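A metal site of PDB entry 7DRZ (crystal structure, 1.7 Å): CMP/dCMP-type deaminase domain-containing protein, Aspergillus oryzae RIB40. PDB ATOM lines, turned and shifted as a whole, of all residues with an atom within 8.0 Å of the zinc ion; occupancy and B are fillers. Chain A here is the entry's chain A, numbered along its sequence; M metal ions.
The zinc ion is bound by ND1 of His 61 (2.0 Å), SG of Cys 112 (2.3 Å) and SG of Cys 102 (2.3 Å).
Of the 26 residues printed, 3 come within 4 Å of the zinc ion.
Along chain A the residues within 4 Å of the zinc ion span positions 61 to 112.
The backbone NH (N) of His 61 lies within hydrogen-bond range of the side-chain amide oxygen (OE1) of Gln 64 (3.0 Å).
OE1 of Glu 63 lies close to SG of Cys 112 (3.5 Å).
The backbone NH (N) of Val 113 sits at hydrogen-bond distance from the backbone carbonyl oxygen (O) of Cys 102, at 2.9 Å.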
ATOM      1  N   PHE A  26      -9.413   5.138 -27.252  1.00  0.00           N
ATOM      2  CA  PHE A  26      -8.809   5.040 -28.574  1.00  0.00           C
ATOM      3  C   PHE A  26      -9.807   4.328 -29.476  1.00  0.00           C
ATOM      4  O   PHE A  26     -10.054   3.126 -29.300  1.00  0.00           O
ATOM      5  CB  PHE A  26      -7.465   4.312 -28.507  1.00  0.00           C
ATOM      6  CG  PHE A  26      -6.342   5.180 -27.986  1.00  0.00           C
ATOM      7  CD1 PHE A  26      -6.275   5.487 -26.632  1.00  0.00           C
ATOM      8  CD2 PHE A  26      -5.385   5.692 -28.843  1.00  0.00           C
ATOM      9  CE1 PHE A  26      -5.260   6.297 -26.147  1.00  0.00           C
ATOM     10  CE2 PHE A  26      -4.367   6.512 -28.358  1.00  0.00           C
ATOM     11  CZ  PHE A  26      -4.303   6.809 -27.004  1.00  0.00           C
ATOM     12  N   VAL A  28     -11.127   2.399 -32.315  1.00  0.00           N
ATOM     13  CA  VAL A  28     -10.523   1.386 -33.164  1.00  0.00           C
ATOM     14  C   VAL A  28     -11.634   0.482 -33.664  1.00  0.00           C
ATOM     15  O   VAL A  28     -12.661   0.297 -32.995  1.00  0.00           O
ATOM     16  CB  VAL A  28      -9.450   0.597 -32.374  1.00  0.00           C
ATOM     17  CG1 VAL A  28      -8.868  -0.535 -33.188  1.00  0.00           C
ATOM     18  CG2 VAL A  28      -8.349   1.546 -31.896  1.00  0.00           C
ATOM     19  N   THR A  53     -14.312  -0.121 -30.535  1.00  0.00           N
ATOM     20  CA  THR A  53     -14.129   0.368 -29.165  1.00  0.00           C
ATOM     21  C   THR A  53     -15.444   0.834 -28.557  1.00  0.00           C
ATOM     22  O   THR A  53     -16.172   1.643 -29.142  1.00  0.00           O
ATOM     23  CB  THR A  53     -13.128   1.520 -29.173  1.00  0.00           C
ATOM     24  OG1 THR A  53     -11.890   1.056 -29.699  1.00  0.00           O
ATOM     25  CG2 THR A  53     -12.931   2.071 -27.756  1.00  0.00           C
ATOM     26  N   THR A  60     -14.259  -1.166 -23.183  1.00  0.00           N
ATOM     27  CA  THR A  60     -13.982  -2.304 -24.063  1.00  0.00           C
ATOM     28  C   THR A  60     -13.216  -1.859 -25.301  1.00  0.00           C
ATOM     29  O   THR A  60     -13.500  -0.811 -25.879  1.00  0.00           O
ATOM     30  CB  THR A  60     -15.283  -2.981 -24.473  1.00  0.00           C
ATOM     31  OG1 THR A  60     -16.169  -2.016 -25.062  1.00  0.00           O
ATOM     32  CG2 THR A  60     -15.976  -3.605 -23.265  1.00  0.00           C
ATOM     33  N   HIS A  61     -12.236  -2.669 -25.711  1.00  0.00           N
ATOM     34  CA  HIS A  61     -11.442  -2.403 -26.897  1.00  0.00           C
ATOM     35  C   HIS A  61     -12.078  -3.088 -28.124  1.00  0.00           C
ATOM     36  O   HIS A  61     -12.984  -3.906 -27.996  1.00  0.00           O
ATOM     37  CB  HIS A  61     -10.000  -2.893 -26.691  1.00  0.00           C
ATOM     38  CG  HIS A  61      -9.191  -1.984 -25.822  1.00  0.00           C
ATOM     39  ND1 HIS A  61      -7.815  -2.090 -25.706  1.00  0.00           N
ATOM     40  CD2 HIS A  61      -9.553  -0.936 -25.039  1.00  0.00           C
ATOM     41  CE1 HIS A  61      -7.371  -1.152 -24.886  1.00  0.00           C
ATOM     42  NE2 HIS A  61      -8.402  -0.440 -24.464  1.00  0.00           N
ATOM     43  N   ALA A  62     -11.595  -2.715 -29.313  1.00  0.00           N
ATOM     44  CA  ALA A  62     -12.209  -3.227 -30.553  1.00  0.00           C
ATOM     45  C   ALA A  62     -12.059  -4.746 -30.670  1.00  0.00           C
ATOM     46  O   ALA A  62     -13.007  -5.446 -31.025  1.00  0.00           O
ATOM     47  CB  ALA A  62     -11.583  -2.546 -31.772  1.00  0.00           C
ATOM     48  N   GLU A  63     -10.849  -5.252 -30.409  1.00  0.00           N
ATOM     49  CA  GLU A  63     -10.598  -6.688 -30.476  1.00  0.00           C
ATOM     50  C   GLU A  63     -11.485  -7.444 -29.499  1.00  0.00           C
ATOM     51  O   GLU A  63     -12.030  -8.509 -29.828  1.00  0.00           O
ATOM     52  CB  GLU A  63      -9.123  -6.982 -30.177  1.00  0.00           C
ATOM     53  CG  GLU A  63      -8.154  -6.453 -31.225  1.00  0.00           C
ATOM     54  CD  GLU A  63      -7.655  -5.022 -30.966  1.00  0.00           C
ATOM     55  OE1 GLU A  63      -8.399  -4.176 -30.432  1.00  0.00           O
ATOM     56  OE2 GLU A  63      -6.483  -4.756 -31.324  1.00  0.00           O
ATOM     57  N   GLN A  64     -11.583  -6.922 -28.280  1.00  0.00           N
ATOM     58  CA  GLN A  64     -12.463  -7.475 -27.252  1.00  0.00           C
ATOM     59  C   GLN A  64     -13.905  -7.525 -27.746  1.00  0.00           C
ATOM     60  O   GLN A  64     -14.575  -8.562 -27.640  1.00  0.00           O
ATOM     61  CB  GLN A  64     -12.328  -6.610 -25.997  1.00  0.00           C
ATOM     62  CG  GLN A  64     -13.202  -6.954 -24.823  1.00  0.00           C
ATOM     63  CD  GLN A  64     -12.970  -5.993 -23.671  1.00  0.00           C
ATOM     64  OE1 GLN A  64     -12.224  -5.009 -23.817  1.00  0.00           O
ATOM     65  NE2 GLN A  64     -13.589  -6.263 -22.533  1.00  0.00           N
ATOM     66  N   VAL A  97      -7.293  -4.844 -37.825  1.00  0.00           N
ATOM     67  CA  VAL A  97      -7.621  -3.880 -36.771  1.00  0.00           C
ATOM     68  C   VAL A  97      -6.827  -2.601 -37.061  1.00  0.00           C
ATOM     69  O   VAL A  97      -5.712  -2.665 -37.571  1.00  0.00           O
ATOM     70  CB  VAL A  97      -7.316  -4.496 -35.388  1.00  0.00           C
ATOM     71  CG1 VAL A  97      -5.827  -4.901 -35.256  1.00  0.00           C
ATOM     72  CG2 VAL A  97      -7.759  -3.561 -34.270  1.00  0.00           C
ATOM     73  N   MET A  99      -5.344  -0.278 -35.264  1.00  0.00           N
ATOM     74  CA  MET A  99      -4.137  -0.079 -34.468  1.00  0.00           C
ATOM     75  C   MET A  99      -3.623  -1.409 -33.924  1.00  0.00           C
ATOM     76  O   MET A  99      -4.400  -2.337 -33.734  1.00  0.00           O
ATOM     77  CB  MET A  99      -4.401   0.877 -33.295  1.00  0.00           C
ATOM     78  CG  MET A  99      -4.899   2.240 -33.733  1.00  0.00           C
ATOM     79  SD  MET A  99      -5.012   3.418 -32.369  1.00  0.00           S
ATOM     80  CE  MET A  99      -3.298   3.894 -32.183  1.00  0.00           C
ATOM     81  N   GLU A 100      -2.316  -1.460 -33.669  1.00  0.00           N
ATOM     82  CA  GLU A 100      -1.680  -2.619 -33.052  1.00  0.00           C
ATOM     83  C   GLU A 100      -2.448  -3.062 -31.805  1.00  0.00           C
ATOM     84  O   GLU A 100      -2.827  -2.210 -30.982  1.00  0.00           O
ATOM     85  CB  GLU A 100      -0.236  -2.243 -32.670  1.00  0.00           C
ATOM     86  CG  GLU A 100       0.531  -3.267 -31.831  1.00  0.00           C
ATOM     87  CD  GLU A 100       1.831  -2.711 -31.293  1.00  0.00           C
ATOM     88  OE1 GLU A 100       2.003  -1.472 -31.330  1.00  0.00           O
ATOM     89  OE2 GLU A 100       2.676  -3.495 -30.813  1.00  0.00           O
ATOM     90  N   PRO A 101      -2.715  -4.354 -31.629  1.00  0.00           N
ATOM     91  CA  PRO A 101      -3.360  -4.801 -30.383  1.00  0.00           C
ATOM     92  C   PRO A 101      -2.481  -4.530 -29.173  1.00  0.00           C
ATOM     93  O   PRO A 101      -1.269  -4.743 -29.199  1.00  0.00           O
ATOM     94  CB  PRO A 101      -3.553  -6.314 -30.602  1.00  0.00           C
ATOM     95  CG  PRO A 101      -2.740  -6.667 -31.821  1.00  0.00           C
ATOM     96  CD  PRO A 101      -2.563  -5.430 -32.625  1.00  0.00           C
ATOM     97  N   CYS A 102      -3.107  -4.052 -28.087  1.00  0.00           N
ATOM     98  CA  CYS A 102      -2.361  -3.688 -26.884  1.00  0.00           C
ATOM     99  C   CYS A 102      -1.873  -4.922 -26.131  1.00  0.00           C
ATOM    100  O   CYS A 102      -2.514  -5.976 -26.142  1.00  0.00           O
ATOM    101  CB  CYS A 102      -3.206  -2.815 -25.950  1.00  0.00           C
ATOM    102  SG  CYS A 102      -4.692  -3.604 -25.206  1.00  0.00           S
ATOM    103  N   GLY A 103      -0.732  -4.770 -25.466  1.00  0.00           N
ATOM    104  CA  GLY A 103      -0.190  -5.827 -24.631  1.00  0.00           C
ATOM    105  C   GLY A 103      -0.218  -5.467 -23.157  1.00  0.00           C
ATOM    106  O   GLY A 103       0.128  -6.288 -22.300  1.00  0.00           O
ATOM    107  N   LYS A 104      -0.646  -4.240 -22.855  1.00  0.00           N
ATOM    108  CA  LYS A 104      -0.717  -3.700 -21.513  1.00  0.00           C
ATOM    109  C   LYS A 104      -1.893  -2.748 -21.426  1.00  0.00           C
ATOM    110  O   LYS A 104      -2.138  -1.980 -22.358  1.00  0.00           O
ATOM    111  CB  LYS A 104       0.568  -2.954 -21.141  1.00  0.00           C
ATOM    112  CG  LYS A 104       0.813  -2.804 -19.659  1.00  0.00           C
ATOM    113  CD  LYS A 104       2.295  -2.618 -19.347  1.00  0.00           C
ATOM    114  CE  LYS A 104       3.122  -3.773 -19.884  1.00  0.00           C
ATOM    115  NZ  LYS A 104       3.247  -4.924 -18.934  1.00  0.00           N
ATOM    116  N   ARG A 105      -2.636  -2.803 -20.325  1.00  0.00           N
ATOM    117  CA  ARG A 105      -3.790  -1.928 -20.133  1.00  0.00           C
ATOM    118  C   ARG A 105      -3.705  -1.233 -18.789  1.00  0.00           C
ATOM    119  O   ARG A 105      -3.403  -1.868 -17.766  1.00  0.00           O
ATOM    120  CB  ARG A 105      -5.107  -2.702 -20.274  1.00  0.00           C
ATOM    121  CG  ARG A 105      -5.426  -3.047 -21.715  1.00  0.00           C
ATOM    122  CD  ARG A 105      -6.851  -3.537 -21.900  1.00  0.00           C
ATOM    123  NE  ARG A 105      -7.844  -2.532 -21.539  1.00  0.00           N
ATOM    124  CZ  ARG A 105      -9.145  -2.643 -21.784  1.00  0.00           C
ATOM    125  NH1 ARG A 105      -9.981  -1.686 -21.406  1.00  0.00           N
ATOM    126  NH2 ARG A 105      -9.611  -3.732 -22.392  1.00  0.00           N
ATOM    127  N   LEU A 110      -7.928  -7.491 -19.293  1.00  0.00           N
ATOM    128  CA  LEU A 110      -6.965  -8.272 -20.067  1.00  0.00           C
ATOM    129  C   LEU A 110      -6.627  -7.529 -21.359  1.00  0.00           C
ATOM    130  O   LEU A 110      -7.535  -7.065 -22.058  1.00  0.00           O
ATOM    131  CB  LEU A 110      -7.548  -9.654 -20.383  1.00  0.00           C
ATOM    132  CG  LEU A 110      -6.627 -10.709 -20.983  1.00  0.00           C
ATOM    133  CD1 LEU A 110      -5.561 -11.130 -19.983  1.00  0.00           C
ATOM    134  CD2 LEU A 110      -7.440 -11.916 -21.448  1.00  0.00           C
ATOM    135  N   PRO A 111      -5.347  -7.401 -21.711  1.00  0.00           N
ATOM    136  CA  PRO A 111      -5.001  -6.712 -22.959  1.00  0.00           C
ATOM    137  C   PRO A 111      -5.381  -7.536 -24.184  1.00  0.00           C
ATOM    138  O   PRO A 111      -5.649  -8.736 -24.100  1.00  0.00           O
ATOM    139  CB  PRO A 111      -3.485  -6.520 -22.872  1.00  0.00           C
ATOM    140  CG  PRO A 111      -3.161  -6.699 -21.401  1.00  0.00           C
ATOM    141  CD  PRO A 111      -4.163  -7.695 -20.899  1.00  0.00           C
ATOM    142  N   CYS A 112      -5.384  -6.860 -25.330  1.00  0.00           N
ATOM    143  CA  CYS A 112      -5.961  -7.448 -26.533  1.00  0.00           C
ATOM    144  C   CYS A 112      -5.102  -8.583 -27.075  1.00  0.00           C
ATOM    145  O   CYS A 112      -5.628  -9.580 -27.591  1.00  0.00           O
ATOM    146  CB  CYS A 112      -6.136  -6.359 -27.585  1.00  0.00           C
ATOM    147  SG  CYS A 112      -7.544  -5.261 -27.206  1.00  0.00           S
ATOM    148  N   VAL A 113      -3.773  -8.449 -26.996  1.00  0.00           N
ATOM    149  CA  VAL A 113      -2.920  -9.517 -27.519  1.00  0.00           C
ATOM    150  C   VAL A 113      -3.169 -10.815 -26.760  1.00  0.00           C
ATOM    151  O   VAL A 113      -3.167 -11.897 -27.345  1.00  0.00           O
ATOM    152  CB  VAL A 113      -1.428  -9.102 -27.458  1.00  0.00           C
ATOM    153  CG1 VAL A 113      -0.525 -10.279 -27.860  1.00  0.00           C
ATOM    154  CG2 VAL A 113      -1.184  -7.940 -28.387  1.00  0.00           C
ATOM    155  N   GLN A 114      -3.403 -10.728 -25.443  1.00  0.00           N
ATOM    156  CA  GLN A 114      -3.683 -11.928 -24.659  1.00  0.00           C
ATOM    157  C   GLN A 114      -5.012 -12.551 -25.066  1.00  0.00           C
ATOM    158  O   GLN A 114      -5.141 -13.788 -25.080  1.00  0.00           O
ATOM    159  CB  GLN A 114      -3.661 -11.596 -23.164  1.00  0.00           C
ATOM    160  CG  GLN A 114      -2.260 -11.345 -22.613  1.00  0.00           C
ATOM    161  CD  GLN A 114      -1.825  -9.901 -22.761  1.00  0.00           C
ATOM    162  OE1 GLN A 114      -2.222  -9.214 -23.696  1.00  0.00           O
ATOM    163  NE2 GLN A 114      -0.976  -9.432 -21.842  1.00  0.00           N
ATOM    164  N   ARG A 115      -6.001 -11.714 -25.390  1.00  0.00           N
ATOM    165  CA  ARG A 115      -7.272 -12.227 -25.905  1.00  0.00           C
ATOM    166  C   ARG A 115      -7.060 -12.958 -27.231  1.00  0.00           C
ATOM    167  O   ARG A 115      -7.687 -14.009 -27.482  1.00  0.00           O
ATOM    168  CB  ARG A 115      -8.278 -11.087 -26.084  1.00  0.00           C
ATOM    169  CG  ARG A 115      -8.714 -10.443 -24.784  1.00  0.00           C
ATOM    170  CD  ARG A 115      -9.621  -9.237 -25.039  1.00  0.00           C
ATOM    171  NE  ARG A 115      -9.842  -8.517 -23.789  1.00  0.00           N
ATOM    172  CZ  ARG A 115     -10.762  -8.848 -22.889  1.00  0.00           C
ATOM    173  NH1 ARG A 115     -10.875  -8.133 -21.773  1.00  0.00           N
ATOM    174  NH2 ARG A 115     -11.581  -9.868 -23.112  1.00  0.00           N
ATOM    175  N   ILE A 116      -6.190 -12.424 -28.077  1.00  0.00           N
ATOM    176  CA  ILE A 116      -5.878 -13.073 -29.353  1.00  0.00           C
ATOM    177  C   ILE A 116      -5.136 -14.389 -29.121  1.00  0.00           C
ATOM    178  O   ILE A 116      -5.488 -15.423 -29.713  1.00  0.00           O
ATOM    179  CB  ILE A 116      -5.062 -12.103 -30.242  1.00  0.00           C
ATOM    180  CG1 ILE A 116      -5.929 -10.899 -30.633  1.00  0.00           C
ATOM    181  CG2 ILE A 116      -4.525 -12.825 -31.495  1.00  0.00           C
ATOM    182  CD1 ILE A 116      -5.124  -9.700 -31.139  1.00  0.00           C
ATOM    183  N   PRO A 137      -0.315   0.907 -30.058  1.00  0.00           N
ATOM    184  CA  PRO A 137      -1.508   0.264 -29.499  1.00  0.00           C
ATOM    185  C   PRO A 137      -2.638   1.259 -29.289  1.00  0.00           C
ATOM    186  O   PRO A 137      -2.450   2.473 -29.273  1.00  0.00           O
ATOM    187  CB  PRO A 137      -1.015  -0.286 -28.163  1.00  0.00           C
ATOM    188  CG  PRO A 137       0.090   0.658 -27.757  1.00  0.00           C
ATOM    189  CD  PRO A 137       0.760   1.049 -29.060  1.00  0.00           C
ATOM    190  N   GLY A 138      -3.842   0.695 -29.122  1.00  0.00           N
ATOM    191  CA  GLY A 138      -5.019   1.479 -28.782  1.00  0.00           C
ATOM    192  C   GLY A 138      -5.073   1.902 -27.328  1.00  0.00           C
ATOM    193  O   GLY A 138      -6.111   1.753 -26.658  1.00  0.00           O
ATOM    194  N   THR A 139      -3.946   2.393 -26.813  1.00  0.00           N
ATOM    195  CA  THR A 139      -3.792   2.860 -25.449  1.00  0.00           C
ATOM    196  C   THR A 139      -2.803   4.018 -25.450  1.00  0.00           C
ATOM    197  O   THR A 139      -2.152   4.294 -26.461  1.00  0.00           O
ATOM    198  CB  THR A 139      -3.243   1.775 -24.510  1.00  0.00           C
ATOM    199  OG1 THR A 139      -1.904   1.472 -24.915  1.00  0.00           O
ATOM    200  CG2 THR A 139      -4.092   0.508 -24.561  1.00  0.00           C
HETATM  201 ZN    ZN M   1      -6.512  -3.316 -26.598  1.00  0.00          ZN
